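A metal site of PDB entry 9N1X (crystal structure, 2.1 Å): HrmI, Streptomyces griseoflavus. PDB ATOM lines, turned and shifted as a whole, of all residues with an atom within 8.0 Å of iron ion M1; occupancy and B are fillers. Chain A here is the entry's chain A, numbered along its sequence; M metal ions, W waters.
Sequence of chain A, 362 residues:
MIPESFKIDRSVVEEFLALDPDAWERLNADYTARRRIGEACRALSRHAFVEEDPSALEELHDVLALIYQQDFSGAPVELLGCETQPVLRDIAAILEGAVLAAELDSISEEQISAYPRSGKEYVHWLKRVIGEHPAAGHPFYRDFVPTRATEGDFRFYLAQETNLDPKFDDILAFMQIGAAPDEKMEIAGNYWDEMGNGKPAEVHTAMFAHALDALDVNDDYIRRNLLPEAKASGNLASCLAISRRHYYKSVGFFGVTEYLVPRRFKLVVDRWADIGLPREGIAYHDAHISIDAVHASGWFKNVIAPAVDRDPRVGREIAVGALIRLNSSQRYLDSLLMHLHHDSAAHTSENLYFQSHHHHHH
O of Tyr 284 sits at hydrogen-bond distance from ND1 of His 288, at 2.8 Å.
Within 4 Å of iron ion M1: Glu 194, His 204 and His 288.
Water W1 is bound to iron ion M1 (1.9 Å).
Iron ion M1 is bound by the side-chain carboxylate (OE2) of Glu 194, at 2.0 Å.
NE2 of His 288 binds iron ion M1.
Water W2 is bound to iron ion M1.
ND1 of His 204 is bound to iron ion M1 (2.3 Å).
Slightly farther from iron ion M1 lies the side-chain carboxylate (OE1) of Glu 194 (2.7 Å).
Water W2 lies within hydrogen-bond range of the side-chain hydroxyl of Tyr 284 (2.8 Å) and the side-chain carboxylate of Glu 194 (3.0 Å).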
ATOM      1  N   ASP A 165      -3.219  29.948 -16.202  1.00  0.00           N
ATOM      2  CA  ASP A 165      -2.005  29.851 -15.382  1.00  0.00           C
ATOM      3  C   ASP A 165      -2.209  29.213 -14.003  1.00  0.00           C
ATOM      4  O   ASP A 165      -1.362  28.388 -13.624  1.00  0.00           O
ATOM      5  CB  ASP A 165      -1.383  31.243 -15.243  1.00  0.00           C
ATOM      6  CG  ASP A 165      -1.065  31.883 -16.578  1.00  0.00           C
ATOM      7  OD1 ASP A 165      -1.909  31.792 -17.492  1.00  0.00           O
ATOM      8  OD2 ASP A 165       0.038  32.461 -16.735  1.00  0.00           O
ATOM      9  N   PHE A 168      -1.718  25.322 -14.446  1.00  0.00           N
ATOM     10  CA  PHE A 168      -0.718  24.806 -15.373  1.00  0.00           C
ATOM     11  C   PHE A 168      -0.090  23.509 -14.864  1.00  0.00           C
ATOM     12  O   PHE A 168       0.166  22.578 -15.631  1.00  0.00           O
ATOM     13  CB  PHE A 168       0.364  25.861 -15.589  1.00  0.00           C
ATOM     14  CG  PHE A 168       0.783  26.031 -17.004  1.00  0.00           C
ATOM     15  CD1 PHE A 168       0.036  26.811 -17.878  1.00  0.00           C
ATOM     16  CD2 PHE A 168       1.937  25.425 -17.475  1.00  0.00           C
ATOM     17  CE1 PHE A 168       0.434  26.971 -19.188  1.00  0.00           C
ATOM     18  CE2 PHE A 168       2.338  25.584 -18.776  1.00  0.00           C
ATOM     19  CZ  PHE A 168       1.585  26.351 -19.650  1.00  0.00           C
ATOM     20  N   ASP A 169       0.210  23.453 -13.562  1.00  0.00           N
ATOM     21  CA  ASP A 169       0.883  22.259 -13.049  1.00  0.00           C
ATOM     22  C   ASP A 169       0.013  21.011 -13.205  1.00  0.00           C
ATOM     23  O   ASP A 169       0.516  19.942 -13.572  1.00  0.00           O
ATOM     24  CB  ASP A 169       1.301  22.456 -11.589  1.00  0.00           C
ATOM     25  CG  ASP A 169       0.219  23.119 -10.720  1.00  0.00           C
ATOM     26  OD1 ASP A 169      -0.996  23.117 -11.079  1.00  0.00           O
ATOM     27  OD2 ASP A 169       0.631  23.626  -9.663  1.00  0.00           O
ATOM     28  N   LEU A 172      -0.267  19.821 -16.829  1.00  0.00           N
ATOM     29  CA  LEU A 172       0.889  19.010 -17.211  1.00  0.00           C
ATOM     30  C   LEU A 172       0.795  17.615 -16.606  1.00  0.00           C
ATOM     31  O   LEU A 172       1.150  16.621 -17.250  1.00  0.00           O
ATOM     32  CB  LEU A 172       2.190  19.685 -16.792  1.00  0.00           C
ATOM     33  CG  LEU A 172       2.505  21.028 -17.450  1.00  0.00           C
ATOM     34  CD1 LEU A 172       3.600  21.739 -16.682  1.00  0.00           C
ATOM     35  CD2 LEU A 172       2.929  20.816 -18.878  1.00  0.00           C
ATOM     36  N   ASN A 190       9.096  19.784 -16.814  1.00  0.00           N
ATOM     37  CA  ASN A 190       8.325  21.016 -16.877  1.00  0.00           C
ATOM     38  C   ASN A 190       7.433  21.157 -15.642  1.00  0.00           C
ATOM     39  O   ASN A 190       7.442  22.196 -14.965  1.00  0.00           O
ATOM     40  CB  ASN A 190       7.513  21.031 -18.175  1.00  0.00           C
ATOM     41  CG  ASN A 190       6.956  22.408 -18.521  1.00  0.00           C
ATOM     42  OD1 ASN A 190       6.408  23.087 -17.659  1.00  0.00           O
ATOM     43  ND2 ASN A 190       7.074  22.802 -19.785  1.00  0.00           N
ATOM     44  N   ASP A 193       9.466  22.058 -12.667  1.00  0.00           N
ATOM     45  CA  ASP A 193       9.757  23.494 -12.663  1.00  0.00           C
ATOM     46  C   ASP A 193       8.549  24.286 -12.145  1.00  0.00           C
ATOM     47  O   ASP A 193       8.705  25.201 -11.344  1.00  0.00           O
ATOM     48  CB  ASP A 193      10.144  23.981 -14.067  1.00  0.00           C
ATOM     49  CG  ASP A 193      11.530  23.526 -14.521  1.00  0.00           C
ATOM     50  OD1 ASP A 193      12.418  23.165 -13.704  1.00  0.00           O
ATOM     51  OD2 ASP A 193      11.745  23.534 -15.759  1.00  0.00           O
ATOM     52  N   GLU A 194       7.343  23.950 -12.619  1.00  0.00           N
ATOM     53  CA  GLU A 194       6.124  24.592 -12.127  1.00  0.00           C
ATOM     54  C   GLU A 194       5.993  24.453 -10.610  1.00  0.00           C
ATOM     55  O   GLU A 194       5.441  25.326  -9.936  1.00  0.00           O
ATOM     56  CB  GLU A 194       4.886  24.005 -12.814  1.00  0.00           C
ATOM     57  CG  GLU A 194       4.739  24.362 -14.300  1.00  0.00           C
ATOM     58  CD  GLU A 194       4.497  25.850 -14.528  1.00  0.00           C
ATOM     59  OE1 GLU A 194       3.575  26.409 -13.883  1.00  0.00           O
ATOM     60  OE2 GLU A 194       5.218  26.472 -15.335  1.00  0.00           O
ATOM     61  N   MET A 195       6.501  23.348 -10.069  1.00  0.00           N
ATOM     62  CA  MET A 195       6.507  23.065  -8.645  1.00  0.00           C
ATOM     63  C   MET A 195       7.730  23.666  -7.949  1.00  0.00           C
ATOM     64  O   MET A 195       8.135  23.182  -6.883  1.00  0.00           O
ATOM     65  CB  MET A 195       6.457  21.539  -8.465  1.00  0.00           C
ATOM     66  CG  MET A 195       5.050  20.861  -8.484  1.00  0.00           C
ATOM     67  SD  MET A 195       3.636  21.781  -7.860  1.00  0.00           S
ATOM     68  CE  MET A 195       3.924  21.447  -6.097  1.00  0.00           C
ATOM     69  N   GLU A 202       9.016  29.229  -4.910  1.00  0.00           N
ATOM     70  CA  GLU A 202       9.144  29.267  -6.359  1.00  0.00           C
ATOM     71  C   GLU A 202       8.033  28.508  -7.097  1.00  0.00           C
ATOM     72  O   GLU A 202       8.110  28.376  -8.321  1.00  0.00           O
ATOM     73  CB  GLU A 202      10.516  28.740  -6.778  1.00  0.00           C
ATOM     74  CG  GLU A 202      11.659  29.722  -6.476  1.00  0.00           C
ATOM     75  CD  GLU A 202      13.035  29.125  -6.681  1.00  0.00           C
ATOM     76  OE1 GLU A 202      13.294  28.543  -7.761  1.00  0.00           O
ATOM     77  OE2 GLU A 202      13.864  29.230  -5.758  1.00  0.00           O
ATOM     78  N   VAL A 203       7.015  28.007  -6.390  1.00  0.00           N
ATOM     79  CA  VAL A 203       5.887  27.362  -7.056  1.00  0.00           C
ATOM     80  C   VAL A 203       5.139  28.404  -7.887  1.00  0.00           C
ATOM     81  O   VAL A 203       4.797  29.482  -7.383  1.00  0.00           O
ATOM     82  CB  VAL A 203       4.955  26.697  -6.034  1.00  0.00           C
ATOM     83  CG1 VAL A 203       3.701  26.141  -6.730  1.00  0.00           C
ATOM     84  CG2 VAL A 203       5.683  25.573  -5.277  1.00  0.00           C
ATOM     85  N   HIS A 204       4.871  28.080  -9.147  1.00  0.00           N
ATOM     86  CA  HIS A 204       4.366  29.093 -10.078  1.00  0.00           C
ATOM     87  C   HIS A 204       2.971  29.586  -9.711  1.00  0.00           C
ATOM     88  O   HIS A 204       2.686  30.772  -9.841  1.00  0.00           O
ATOM     89  CB  HIS A 204       4.401  28.560 -11.498  1.00  0.00           C
ATOM     90  CG  HIS A 204       5.770  28.504 -12.071  1.00  0.00           C
ATOM     91  ND1 HIS A 204       6.024  28.077 -13.358  1.00  0.00           N
ATOM     92  CD2 HIS A 204       6.970  28.794 -11.528  1.00  0.00           C
ATOM     93  CE1 HIS A 204       7.322  28.112 -13.580  1.00  0.00           C
ATOM     94  NE2 HIS A 204       7.918  28.558 -12.487  1.00  0.00           N
ATOM     95  N   THR A 205       2.060  28.696  -9.288  1.00  0.00           N
ATOM     96  CA  THR A 205       0.740  29.169  -8.889  1.00  0.00           C
ATOM     97  C   THR A 205       0.845  30.143  -7.718  1.00  0.00           C
ATOM     98  O   THR A 205       0.070  31.102  -7.628  1.00  0.00           O
ATOM     99  CB  THR A 205      -0.183  28.022  -8.503  1.00  0.00           C
ATOM    100  OG1 THR A 205       0.423  27.239  -7.466  1.00  0.00           O
ATOM    101  CG2 THR A 205      -0.487  27.130  -9.689  1.00  0.00           C
ATOM    102  N   PHE A 208       1.992  33.389  -9.098  1.00  0.00           N
ATOM    103  CA  PHE A 208       0.913  34.028  -9.849  1.00  0.00           C
ATOM    104  C   PHE A 208      -0.084  34.698  -8.914  1.00  0.00           C
ATOM    105  O   PHE A 208      -0.568  35.800  -9.191  1.00  0.00           O
ATOM    106  CB  PHE A 208       0.192  33.004 -10.727  1.00  0.00           C
ATOM    107  CG  PHE A 208      -0.806  33.612 -11.669  1.00  0.00           C
ATOM    108  CD1 PHE A 208      -0.382  34.268 -12.813  1.00  0.00           C
ATOM    109  CD2 PHE A 208      -2.166  33.518 -11.435  1.00  0.00           C
ATOM    110  CE1 PHE A 208      -1.292  34.811 -13.705  1.00  0.00           C
ATOM    111  CE2 PHE A 208      -3.097  34.063 -12.318  1.00  0.00           C
ATOM    112  CZ  PHE A 208      -2.645  34.714 -13.452  1.00  0.00           C
ATOM    113  N   GLU A 258       3.828  27.591 -24.533  1.00  0.00           N
ATOM    114  CA  GLU A 258       5.210  27.788 -24.122  1.00  0.00           C
ATOM    115  C   GLU A 258       5.971  28.630 -25.119  1.00  0.00           C
ATOM    116  O   GLU A 258       6.746  29.520 -24.747  1.00  0.00           O
ATOM    117  CB  GLU A 258       5.903  26.425 -23.946  1.00  0.00           C
ATOM    118  CG  GLU A 258       5.208  25.483 -22.951  1.00  0.00           C
ATOM    119  CD  GLU A 258       5.214  26.045 -21.541  1.00  0.00           C
ATOM    120  OE1 GLU A 258       4.386  26.944 -21.257  1.00  0.00           O
ATOM    121  OE2 GLU A 258       6.046  25.609 -20.718  1.00  0.00           O
ATOM    122  N   VAL A 261       4.953  32.498 -24.772  1.00  0.00           N
ATOM    123  CA  VAL A 261       5.004  33.213 -23.479  1.00  0.00           C
ATOM    124  C   VAL A 261       6.150  34.209 -23.415  1.00  0.00           C
ATOM    125  O   VAL A 261       5.931  35.341 -22.949  1.00  0.00           O
ATOM    126  CB  VAL A 261       5.005  32.218 -22.317  1.00  0.00           C
ATOM    127  CG1 VAL A 261       5.560  32.879 -21.045  1.00  0.00           C
ATOM    128  CG2 VAL A 261       3.594  31.706 -22.071  1.00  0.00           C
ATOM    129  N   PHE A 265       5.279  37.951 -22.343  1.00  0.00           N
ATOM    130  CA  PHE A 265       5.568  38.340 -20.958  1.00  0.00           C
ATOM    131  C   PHE A 265       6.620  39.440 -20.902  1.00  0.00           C
ATOM    132  O   PHE A 265       6.579  40.285 -19.995  1.00  0.00           O
ATOM    133  CB  PHE A 265       6.019  37.130 -20.155  1.00  0.00           C
ATOM    134  CG  PHE A 265       4.883  36.283 -19.625  1.00  0.00           C
ATOM    135  CD1 PHE A 265       3.614  36.343 -20.191  1.00  0.00           C
ATOM    136  CD2 PHE A 265       5.091  35.430 -18.547  1.00  0.00           C
ATOM    137  CE1 PHE A 265       2.567  35.566 -19.682  1.00  0.00           C
ATOM    138  CE2 PHE A 265       4.043  34.646 -18.049  1.00  0.00           C
ATOM    139  CZ  PHE A 265       2.791  34.713 -18.621  1.00  0.00           C
ATOM    140  N   TYR A 284       6.629  36.824 -11.167  1.00  0.00           N
ATOM    141  CA  TYR A 284       6.018  35.748 -11.945  1.00  0.00           C
ATOM    142  C   TYR A 284       6.396  35.837 -13.427  1.00  0.00           C
ATOM    143  O   TYR A 284       6.823  34.840 -14.022  1.00  0.00           O
ATOM    144  CB  TYR A 284       4.494  35.793 -11.794  1.00  0.00           C
ATOM    145  CG  TYR A 284       3.793  34.767 -12.647  1.00  0.00           C
ATOM    146  CD1 TYR A 284       3.727  33.429 -12.249  1.00  0.00           C
ATOM    147  CD2 TYR A 284       3.198  35.108 -13.876  1.00  0.00           C
ATOM    148  CE1 TYR A 284       3.107  32.480 -13.019  1.00  0.00           C
ATOM    149  CE2 TYR A 284       2.575  34.155 -14.667  1.00  0.00           C
ATOM    150  CZ  TYR A 284       2.529  32.829 -14.220  1.00  0.00           C
ATOM    151  OH  TYR A 284       1.921  31.851 -14.957  1.00  0.00           O
ATOM    152  N   ALA A 287      10.307  35.264 -14.160  1.00  0.00           N
ATOM    153  CA  ALA A 287      10.674  33.860 -14.226  1.00  0.00           C
ATOM    154  C   ALA A 287      10.447  33.319 -15.623  1.00  0.00           C
ATOM    155  O   ALA A 287      11.393  32.867 -16.299  1.00  0.00           O
ATOM    156  CB  ALA A 287       9.860  33.064 -13.189  1.00  0.00           C
ATOM    157  N   HIS A 288       9.219  33.452 -16.136  1.00  0.00           N
ATOM    158  CA  HIS A 288       8.809  32.755 -17.351  1.00  0.00           C
ATOM    159  C   HIS A 288       9.536  33.247 -18.591  1.00  0.00           C
ATOM    160  O   HIS A 288       9.716  32.472 -19.538  1.00  0.00           O
ATOM    161  CB  HIS A 288       7.308  32.885 -17.530  1.00  0.00           C
ATOM    162  CG  HIS A 288       6.536  32.041 -16.573  1.00  0.00           C
ATOM    163  ND1 HIS A 288       6.397  32.384 -15.250  1.00  0.00           N
ATOM    164  CD2 HIS A 288       5.959  30.831 -16.714  1.00  0.00           C
ATOM    165  CE1 HIS A 288       5.704  31.444 -14.626  1.00  0.00           C
ATOM    166  NE2 HIS A 288       5.436  30.481 -15.492  1.00  0.00           N
ATOM    167  N   ILE A 291      12.533  31.087 -18.376  1.00  0.00           N
ATOM    168  CA  ILE A 291      12.205  29.664 -18.221  1.00  0.00           C
ATOM    169  C   ILE A 291      11.545  29.120 -19.483  1.00  0.00           C
ATOM    170  O   ILE A 291      11.877  28.031 -19.963  1.00  0.00           O
ATOM    171  CB  ILE A 291      11.315  29.470 -16.977  1.00  0.00           C
ATOM    172  CG1 ILE A 291      12.121  29.691 -15.695  1.00  0.00           C
ATOM    173  CG2 ILE A 291      10.694  28.097 -16.971  1.00  0.00           C
ATOM    174  N   ASP A 292      10.637  29.886 -20.079  1.00  0.00           N
ATOM    175  CA  ASP A 292       9.821  29.337 -21.151  1.00  0.00           C
ATOM    176  C   ASP A 292      10.507  29.348 -22.516  1.00  0.00           C
ATOM    177  O   ASP A 292      10.016  28.679 -23.433  1.00  0.00           O
ATOM    178  CB  ASP A 292       8.476  30.060 -21.194  1.00  0.00           C
ATOM    179  CG  ASP A 292       7.475  29.413 -20.261  1.00  0.00           C
ATOM    180  OD1 ASP A 292       7.694  28.226 -19.898  1.00  0.00           O
ATOM    181  OD2 ASP A 292       6.485  30.065 -19.899  1.00  0.00           O
ATOM    182  N   HIS A 295      11.608  25.894 -21.863  1.00  0.00           N
ATOM    183  CA  HIS A 295      10.466  24.983 -21.943  1.00  0.00           C
ATOM    184  C   HIS A 295      10.016  24.793 -23.390  1.00  0.00           C
ATOM    185  O   HIS A 295       9.694  23.669 -23.798  1.00  0.00           O
ATOM    186  CB  HIS A 295       9.309  25.479 -21.079  1.00  0.00           C
ATOM    187  CG  HIS A 295       9.468  25.179 -19.619  1.00  0.00           C
ATOM    188  ND1 HIS A 295       8.565  25.590 -18.674  1.00  0.00           N
ATOM    189  CD2 HIS A 295      10.454  24.523 -18.944  1.00  0.00           C
ATOM    190  CE1 HIS A 295       8.968  25.196 -17.480  1.00  0.00           C
ATOM    191  NE2 HIS A 295      10.113  24.553 -17.616  1.00  0.00           N
HETATM  192 FE    FE M   1       4.751  28.422 -15.185  1.00  0.00          FE
HETATM  193 FE    FE M   2       6.637  26.726 -18.887  1.00  0.00          FE
HETATM  194  O   HOH W   1       3.439  28.407 -16.536  1.00  0.00           O
HETATM  195  O   HOH W   2       2.833  29.285 -14.400  1.00  0.00           O
HETATM  196  O   HOH W   3       7.065  27.924 -17.065  1.00  0.00           O
